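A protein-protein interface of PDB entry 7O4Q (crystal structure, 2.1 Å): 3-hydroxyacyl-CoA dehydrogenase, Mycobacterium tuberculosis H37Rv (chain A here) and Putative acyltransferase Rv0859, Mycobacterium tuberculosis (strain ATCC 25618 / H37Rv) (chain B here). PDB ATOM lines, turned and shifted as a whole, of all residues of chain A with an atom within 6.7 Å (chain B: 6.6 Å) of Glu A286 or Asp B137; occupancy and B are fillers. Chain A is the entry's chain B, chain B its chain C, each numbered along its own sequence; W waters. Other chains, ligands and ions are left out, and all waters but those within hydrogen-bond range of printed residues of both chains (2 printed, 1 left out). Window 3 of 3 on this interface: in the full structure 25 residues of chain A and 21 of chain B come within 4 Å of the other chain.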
ATOM      1  N   ILE A 178     -16.686   2.298  -0.420  1.00  0.00           N
ATOM      2  CA  ILE A 178     -17.970   2.990  -0.512  1.00  0.00           C
ATOM      3  C   ILE A 178     -17.826   4.452  -0.105  1.00  0.00           C
ATOM      4  O   ILE A 178     -18.248   5.361  -0.829  1.00  0.00           O
ATOM      5  CB  ILE A 178     -19.028   2.267   0.340  1.00  0.00           C
ATOM      6  CG1 ILE A 178     -19.325   0.883  -0.244  1.00  0.00           C
ATOM      7  CG2 ILE A 178     -20.299   3.103   0.445  1.00  0.00           C
ATOM      8  CD1 ILE A 178     -20.150   0.001   0.670  1.00  0.00           C
ATOM      9  N   PRO A 249     -20.355  -3.924   3.018  1.00  0.00           N
ATOM     10  CA  PRO A 249     -21.435  -3.653   3.983  1.00  0.00           C
ATOM     11  C   PRO A 249     -21.562  -4.696   5.082  1.00  0.00           C
ATOM     12  O   PRO A 249     -22.110  -4.384   6.146  1.00  0.00           O
ATOM     13  CB  PRO A 249     -22.689  -3.614   3.099  1.00  0.00           C
ATOM     14  CG  PRO A 249     -22.181  -3.137   1.779  1.00  0.00           C
ATOM     15  CD  PRO A 249     -20.818  -3.766   1.624  1.00  0.00           C
ATOM     16  N   LEU A 258     -22.189   2.684   8.465  1.00  0.00           N
ATOM     17  CA  LEU A 258     -23.049   2.712   7.285  1.00  0.00           C
ATOM     18  C   LEU A 258     -24.413   3.360   7.520  1.00  0.00           C
ATOM     19  O   LEU A 258     -24.906   4.029   6.594  1.00  0.00           O
ATOM     20  CB  LEU A 258     -23.206   1.283   6.751  1.00  0.00           C
ATOM     21  CG  LEU A 258     -23.908   1.051   5.412  1.00  0.00           C
ATOM     22  CD1 LEU A 258     -23.228   1.831   4.301  1.00  0.00           C
ATOM     23  CD2 LEU A 258     -23.917  -0.433   5.087  1.00  0.00           C
ATOM     24  N   PRO A 262     -26.712   7.742   4.724  1.00  0.00           N
ATOM     25  CA  PRO A 262     -27.884   8.486   4.234  1.00  0.00           C
ATOM     26  C   PRO A 262     -28.224   9.700   5.080  1.00  0.00           C
ATOM     27  O   PRO A 262     -28.717  10.697   4.538  1.00  0.00           O
ATOM     28  CB  PRO A 262     -29.011   7.441   4.266  1.00  0.00           C
ATOM     29  CG  PRO A 262     -28.314   6.124   4.289  1.00  0.00           C
ATOM     30  CD  PRO A 262     -27.071   6.358   5.084  1.00  0.00           C
ATOM     31  N   LEU A 281     -25.713   6.640  -3.947  1.00  0.00           N
ATOM     32  CA  LEU A 281     -25.357   5.942  -2.715  1.00  0.00           C
ATOM     33  C   LEU A 281     -25.983   4.552  -2.667  1.00  0.00           C
ATOM     34  O   LEU A 281     -25.335   3.587  -2.244  1.00  0.00           O
ATOM     35  CB  LEU A 281     -25.779   6.770  -1.500  1.00  0.00           C
ATOM     36  CG  LEU A 281     -25.506   6.154  -0.122  1.00  0.00           C
ATOM     37  CD1 LEU A 281     -24.029   5.821   0.051  1.00  0.00           C
ATOM     38  CD2 LEU A 281     -25.986   7.080   0.988  1.00  0.00           C
ATOM     39  N   ALA A 282     -27.241   4.431  -3.097  1.00  0.00           N
ATOM     40  CA  ALA A 282     -27.894   3.124  -3.107  1.00  0.00           C
ATOM     41  C   ALA A 282     -27.183   2.171  -4.057  1.00  0.00           C
ATOM     42  O   ALA A 282     -26.865   1.033  -3.693  1.00  0.00           O
ATOM     43  CB  ALA A 282     -29.367   3.272  -3.487  1.00  0.00           C
ATOM     44  N   ALA A 283     -26.913   2.627  -5.283  1.00  0.00           N
ATOM     45  CA  ALA A 283     -26.193   1.796  -6.242  1.00  0.00           C
ATOM     46  C   ALA A 283     -24.818   1.409  -5.716  1.00  0.00           C
ATOM     47  O   ALA A 283     -24.376   0.267  -5.894  1.00  0.00           O
ATOM     48  CB  ALA A 283     -26.072   2.527  -7.581  1.00  0.00           C
ATOM     49  N   ALA A 284     -24.133   2.340  -5.047  1.00  0.00           N
ATOM     50  CA  ALA A 284     -22.786   2.065  -4.556  1.00  0.00           C
ATOM     51  C   ALA A 284     -22.796   0.966  -3.501  1.00  0.00           C
ATOM     52  O   ALA A 284     -21.970   0.046  -3.537  1.00  0.00           O
ATOM     53  CB  ALA A 284     -22.165   3.342  -3.991  1.00  0.00           C
ATOM     54  N   VAL A 285     -23.728   1.042  -2.551  1.00  0.00           N
ATOM     55  CA  VAL A 285     -23.753   0.079  -1.456  1.00  0.00           C
ATOM     56  C   VAL A 285     -24.334  -1.253  -1.913  1.00  0.00           C
ATOM     57  O   VAL A 285     -23.814  -2.320  -1.564  1.00  0.00           O
ATOM     58  CB  VAL A 285     -24.526   0.660  -0.261  1.00  0.00           C
ATOM     59  CG1 VAL A 285     -24.624  -0.363   0.862  1.00  0.00           C
ATOM     60  CG2 VAL A 285     -23.851   1.940   0.227  1.00  0.00           C
ATOM     61  N   GLU A 286     -25.424  -1.219  -2.687  1.00  0.00           N
ATOM     62  CA  GLU A 286     -25.992  -2.460  -3.206  1.00  0.00           C
ATOM     63  C   GLU A 286     -24.998  -3.178  -4.109  1.00  0.00           C
ATOM     64  O   GLU A 286     -24.929  -4.414  -4.116  1.00  0.00           O
ATOM     65  CB  GLU A 286     -27.296  -2.174  -3.958  1.00  0.00           C
ATOM     66  CG  GLU A 286     -28.409  -1.621  -3.077  1.00  0.00           C
ATOM     67  CD  GLU A 286     -29.678  -1.299  -3.852  1.00  0.00           C
ATOM     68  OE1 GLU A 286     -29.974  -2.000  -4.841  1.00  0.00           O
ATOM     69  OE2 GLU A 286     -30.384  -0.345  -3.464  1.00  0.00           O
ATOM     70  N   GLY A 287     -24.210  -2.416  -4.871  1.00  0.00           N
ATOM     71  CA  GLY A 287     -23.206  -3.023  -5.723  1.00  0.00           C
ATOM     72  C   GLY A 287     -22.061  -3.639  -4.948  1.00  0.00           C
ATOM     73  O   GLY A 287     -21.486  -4.641  -5.380  1.00  0.00           O
ATOM     74  N   ALA A 288     -21.710  -3.055  -3.801  1.00  0.00           N
ATOM     75  CA  ALA A 288     -20.635  -3.598  -2.979  1.00  0.00           C
ATOM     76  C   ALA A 288     -21.007  -4.918  -2.313  1.00  0.00           C
ATOM     77  O   ALA A 288     -20.120  -5.592  -1.785  1.00  0.00           O
ATOM     78  CB  ALA A 288     -20.223  -2.578  -1.916  1.00  0.00           C
ATOM     79  N   GLN A 289     -22.284  -5.304  -2.332  1.00  0.00           N
ATOM     80  CA  GLN A 289     -22.741  -6.541  -1.712  1.00  0.00           C
ATOM     81  C   GLN A 289     -22.676  -7.748  -2.633  1.00  0.00           C
ATOM     82  O   GLN A 289     -22.804  -8.880  -2.153  1.00  0.00           O
ATOM     83  CB  GLN A 289     -24.182  -6.391  -1.222  1.00  0.00           C
ATOM     84  CG  GLN A 289     -24.362  -5.421  -0.080  1.00  0.00           C
ATOM     85  CD  GLN A 289     -25.803  -5.347   0.370  1.00  0.00           C
ATOM     86  OE1 GLN A 289     -26.594  -4.580  -0.175  1.00  0.00           O
ATOM     87  NE2 GLN A 289     -26.157  -6.157   1.361  1.00  0.00           N
ATOM     88  N   VAL A 290     -22.499  -7.549  -3.936  1.00  0.00           N
ATOM     89  CA  VAL A 290     -22.590  -8.622  -4.911  1.00  0.00           C
ATOM     90  C   VAL A 290     -21.344  -8.605  -5.790  1.00  0.00           C
ATOM     91  O   VAL A 290     -20.487  -7.730  -5.674  1.00  0.00           O
ATOM     92  CB  VAL A 290     -23.869  -8.518  -5.766  1.00  0.00           C
ATOM     93  CG1 VAL A 290     -25.095  -8.813  -4.915  1.00  0.00           C
ATOM     94  CG2 VAL A 290     -23.971  -7.130  -6.386  1.00  0.00           C
ATOM     95  N   THR A 294     -22.983  -8.330 -11.370  1.00  0.00           N
ATOM     96  CA  THR A 294     -24.283  -8.007 -10.786  1.00  0.00           C
ATOM     97  C   THR A 294     -24.335  -6.552 -10.335  1.00  0.00           C
ATOM     98  O   THR A 294     -25.356  -5.875 -10.513  1.00  0.00           O
ATOM     99  CB  THR A 294     -24.580  -8.943  -9.612  1.00  0.00           C
ATOM    100  OG1 THR A 294     -24.518 -10.304 -10.055  1.00  0.00           O
ATOM    101  CG2 THR A 294     -25.965  -8.668  -9.040  1.00  0.00           C
ATOM    102  N   ALA A 295     -23.246  -6.059  -9.741  1.00  0.00           N
ATOM    103  CA  ALA A 295     -23.182  -4.661  -9.332  1.00  0.00           C
ATOM    104  C   ALA A 295     -23.387  -3.733 -10.521  1.00  0.00           C
ATOM    105  O   ALA A 295     -24.109  -2.734 -10.424  1.00  0.00           O
ATOM    106  CB  ALA A 295     -21.839  -4.381  -8.656  1.00  0.00           C
ATOM    107  N   ILE A 298     -27.094  -3.568 -11.511  1.00  0.00           N
ATOM    108  CA  ILE A 298     -27.808  -2.725 -10.554  1.00  0.00           C
ATOM    109  C   ILE A 298     -27.580  -1.255 -10.878  1.00  0.00           C
ATOM    110  O   ILE A 298     -28.513  -0.442 -10.855  1.00  0.00           O
ATOM    111  CB  ILE A 298     -27.370  -3.052  -9.115  1.00  0.00           C
ATOM    112  CG1 ILE A 298     -27.748  -4.486  -8.740  1.00  0.00           C
ATOM    113  CG2 ILE A 298     -27.974  -2.055  -8.134  1.00  0.00           C
ATOM    114  CD1 ILE A 298     -27.153  -4.935  -7.412  1.00  0.00           C
ATOM    115  N   TYR A 302     -30.467   1.856 -11.801  1.00  0.00           N
ATOM    116  CA  TYR A 302     -30.579   3.154 -11.145  1.00  0.00           C
ATOM    117  C   TYR A 302     -30.358   4.292 -12.133  1.00  0.00           C
ATOM    118  O   TYR A 302     -31.010   5.339 -12.039  1.00  0.00           O
ATOM    119  CB  TYR A 302     -29.592   3.247  -9.980  1.00  0.00           C
ATOM    120  CG  TYR A 302     -30.137   2.690  -8.682  1.00  0.00           C
ATOM    121  CD1 TYR A 302     -31.101   3.383  -7.959  1.00  0.00           C
ATOM    122  CD2 TYR A 302     -29.693   1.470  -8.183  1.00  0.00           C
ATOM    123  CE1 TYR A 302     -31.607   2.879  -6.773  1.00  0.00           C
ATOM    124  CE2 TYR A 302     -30.192   0.958  -6.993  1.00  0.00           C
ATOM    125  CZ  TYR A 302     -31.150   1.665  -6.297  1.00  0.00           C
ATOM    126  OH  TYR A 302     -31.651   1.163  -5.116  1.00  0.00           O
ATOM    127  N   GLY B 132     -29.654  -5.293   9.139  1.00  0.00           N
ATOM    128  CA  GLY B 132     -31.010  -4.876   8.823  1.00  0.00           C
ATOM    129  C   GLY B 132     -31.043  -3.780   7.776  1.00  0.00           C
ATOM    130  O   GLY B 132     -30.153  -2.931   7.693  1.00  0.00           O
ATOM    131  N   ALA B 133     -32.102  -3.783   6.964  1.00  0.00           N
ATOM    132  CA  ALA B 133     -32.173  -2.856   5.839  1.00  0.00           C
ATOM    133  C   ALA B 133     -32.551  -1.446   6.280  1.00  0.00           C
ATOM    134  O   ALA B 133     -32.063  -0.467   5.703  1.00  0.00           O
ATOM    135  CB  ALA B 133     -33.161  -3.373   4.792  1.00  0.00           C
ATOM    136  N   MET B 134     -33.412  -1.316   7.296  1.00  0.00           N
ATOM    137  CA  MET B 134     -33.824   0.008   7.757  1.00  0.00           C
ATOM    138  C   MET B 134     -32.630   0.877   8.134  1.00  0.00           C
ATOM    139  O   MET B 134     -32.689   2.104   7.995  1.00  0.00           O
ATOM    140  CB  MET B 134     -34.771  -0.113   8.951  1.00  0.00           C
ATOM    141  CG  MET B 134     -36.229  -0.312   8.581  1.00  0.00           C
ATOM    142  SD  MET B 134     -37.295  -0.347  10.037  1.00  0.00           S
ATOM    143  CE  MET B 134     -36.767  -1.877  10.805  1.00  0.00           C
ATOM    144  N   GLY B 135     -31.546   0.267   8.607  1.00  0.00           N
ATOM    145  CA  GLY B 135     -30.358   1.016   8.961  1.00  0.00           C
ATOM    146  C   GLY B 135     -29.263   0.945   7.916  1.00  0.00           C
ATOM    147  O   GLY B 135     -28.658   1.967   7.579  1.00  0.00           O
ATOM    148  N   LEU B 136     -29.013  -0.252   7.380  1.00  0.00           N
ATOM    149  CA  LEU B 136     -27.852  -0.490   6.530  1.00  0.00           C
ATOM    150  C   LEU B 136     -28.126  -0.365   5.035  1.00  0.00           C
ATOM    151  O   LEU B 136     -27.168  -0.260   4.262  1.00  0.00           O
ATOM    152  CB  LEU B 136     -27.268  -1.882   6.815  1.00  0.00           C
ATOM    153  CG  LEU B 136     -26.702  -2.073   8.227  1.00  0.00           C
ATOM    154  CD1 LEU B 136     -26.253  -3.509   8.453  1.00  0.00           C
ATOM    155  CD2 LEU B 136     -25.553  -1.111   8.472  1.00  0.00           C
ATOM    156  N   ASP B 137     -29.387  -0.381   4.600  1.00  0.00           N
ATOM    157  CA  ASP B 137     -29.698  -0.200   3.183  1.00  0.00           C
ATOM    158  C   ASP B 137     -29.969   1.274   2.910  1.00  0.00           C
ATOM    159  O   ASP B 137     -30.940   1.822   3.448  1.00  0.00           O
ATOM    160  CB  ASP B 137     -30.900  -1.039   2.775  1.00  0.00           C
ATOM    161  CG  ASP B 137     -31.236  -0.902   1.295  1.00  0.00           C
ATOM    162  OD1 ASP B 137     -30.335  -1.114   0.456  1.00  0.00           O
ATOM    163  OD2 ASP B 137     -32.403  -0.596   0.968  1.00  0.00           O
ATOM    164  N   PRO B 138     -29.151   1.948   2.094  1.00  0.00           N
ATOM    165  CA  PRO B 138     -29.290   3.411   1.965  1.00  0.00           C
ATOM    166  C   PRO B 138     -30.638   3.861   1.433  1.00  0.00           C
ATOM    167  O   PRO B 138     -31.205   4.829   1.955  1.00  0.00           O
ATOM    168  CB  PRO B 138     -28.153   3.786   1.003  1.00  0.00           C
ATOM    169  CG  PRO B 138     -27.186   2.670   1.097  1.00  0.00           C
ATOM    170  CD  PRO B 138     -27.996   1.433   1.341  1.00  0.00           C
ATOM    171  N   ALA B 139     -31.169   3.194   0.403  1.00  0.00           N
ATOM    172  CA  ALA B 139     -32.474   3.579  -0.125  1.00  0.00           C
ATOM    173  C   ALA B 139     -33.552   3.479   0.946  1.00  0.00           C
ATOM    174  O   ALA B 139     -34.403   4.369   1.069  1.00  0.00           O
ATOM    175  CB  ALA B 139     -32.833   2.714  -1.332  1.00  0.00           C
ATOM    176  N   THR B 140     -33.521   2.409   1.744  1.00  0.00           N
ATOM    177  CA  THR B 140     -34.504   2.247   2.808  1.00  0.00           C
ATOM    178  C   THR B 140     -34.249   3.229   3.943  1.00  0.00           C
ATOM    179  O   THR B 140     -35.186   3.843   4.466  1.00  0.00           O
ATOM    180  CB  THR B 140     -34.478   0.810   3.326  1.00  0.00           C
ATOM    181  OG1 THR B 140     -34.609  -0.096   2.223  1.00  0.00           O
ATOM    182  CG2 THR B 140     -35.614   0.573   4.306  1.00  0.00           C
ATOM    183  N   ASN B 141     -32.985   3.381   4.340  1.00  0.00           N
ATOM    184  CA  ASN B 141     -32.629   4.314   5.403  1.00  0.00           C
ATOM    185  C   ASN B 141     -33.011   5.743   5.025  1.00  0.00           C
ATOM    186  O   ASN B 141     -33.599   6.477   5.829  1.00  0.00           O
ATOM    187  CB  ASN B 141     -31.128   4.191   5.688  1.00  0.00           C
ATOM    188  CG  ASN B 141     -30.652   5.096   6.808  1.00  0.00           C
ATOM    189  OD1 ASN B 141     -30.895   6.306   6.806  1.00  0.00           O
ATOM    190  ND2 ASN B 141     -29.941   4.511   7.766  1.00  0.00           N
ATOM    191  N   TYR B 142     -32.682   6.151   3.799  1.00  0.00           N
ATOM    192  CA  TYR B 142     -32.972   7.511   3.353  1.00  0.00           C
ATOM    193  C   TYR B 142     -34.471   7.782   3.362  1.00  0.00           C
ATOM    194  O   TYR B 142     -34.929   8.786   3.921  1.00  0.00           O
ATOM    195  CB  TYR B 142     -32.387   7.720   1.957  1.00  0.00           C
ATOM    196  CG  TYR B 142     -32.366   9.143   1.448  1.00  0.00           C
ATOM    197  CD1 TYR B 142     -33.486   9.706   0.847  1.00  0.00           C
ATOM    198  CD2 TYR B 142     -31.211   9.910   1.528  1.00  0.00           C
ATOM    199  CE1 TYR B 142     -33.463  11.001   0.362  1.00  0.00           C
ATOM    200  CE2 TYR B 142     -31.177  11.206   1.041  1.00  0.00           C
ATOM    201  CZ  TYR B 142     -32.306  11.746   0.463  1.00  0.00           C
ATOM    202  OH  TYR B 142     -32.276  13.034  -0.017  1.00  0.00           O
HETATM  203  O   HOH W   1     -28.929  -3.772   0.970  1.00  0.00           O
HETATM  204  O   HOH W   2     -30.026   1.001  -1.167  1.00  0.00           O
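OD2 of Asp B137 sits at hydrogen-bond distance from OG1 of Thr B140 (2.6 Å).
O of Gly B135 is in hydrogen-bond range of ND2 of Asn B141 (2.9 Å).
The side-chain hydroxyl (OH) of Tyr A302 lies within hydrogen-bond range of the side-chain carboxylate (OE2) of Glu A286, 2.6 Å away.
Leu A258 touches Leu B136 (CD2 to O, 3.4 Å).
Pro B138 touches Pro A262 (CA to CG, 3.7 Å).
Pro A262 touches Asn B141 (CB to OD1, 3.4 Å).
Pro A262 touches Tyr B142 (CB to N, 3.9 Å).
Leu A281 touches Pro B138.
Pro B138 touches Val A285 (CG to CG2, 3.5 Å).
Glu A286 touches Asp B137.
Printed residues of chain B within 4 Å of Leu A258: Leu B136.
Thr A294 touches none of the printed residues of chain B.
Of the printed residues of chain A, Leu B136 touches Leu A258 (3.4 Å).
Of the printed residues of chain A, Asp B137 touches Glu A286 (3.995 Å).
Of the printed residues of chain A, Pro B138 touches Pro A262, Leu A281 and Val A285.
The nearest printed residue of chain B that does not touch Glu A286 is Ala B139 (4.5 Å).
Printed residues of chain B that touch a printed residue of chain A: Leu B136, Asp B137, Pro B138, Asn B141 and Tyr B142.
Hydrophobic or aromatic side chains of chain B that line the printed part of chain A: Leu B136, Pro B138 and Tyr B142.
Of the 18 printed residues of chain A, 5 touch a printed residue of chain B.
Among the printed residues, 7 pairs touch across the chains.
Water W2 lies within hydrogen-bond range of OD1 of Asp B137 (2.7 Å), OE2 of Glu A286 (2.7 Å) and N of Ala B139 (2.9 Å).
Water W1 lies within hydrogen-bond range of the side-chain amide oxygen of Gln A289 (2.7 Å) and the side-chain carboxylate of Asp B137 (3.1 Å).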
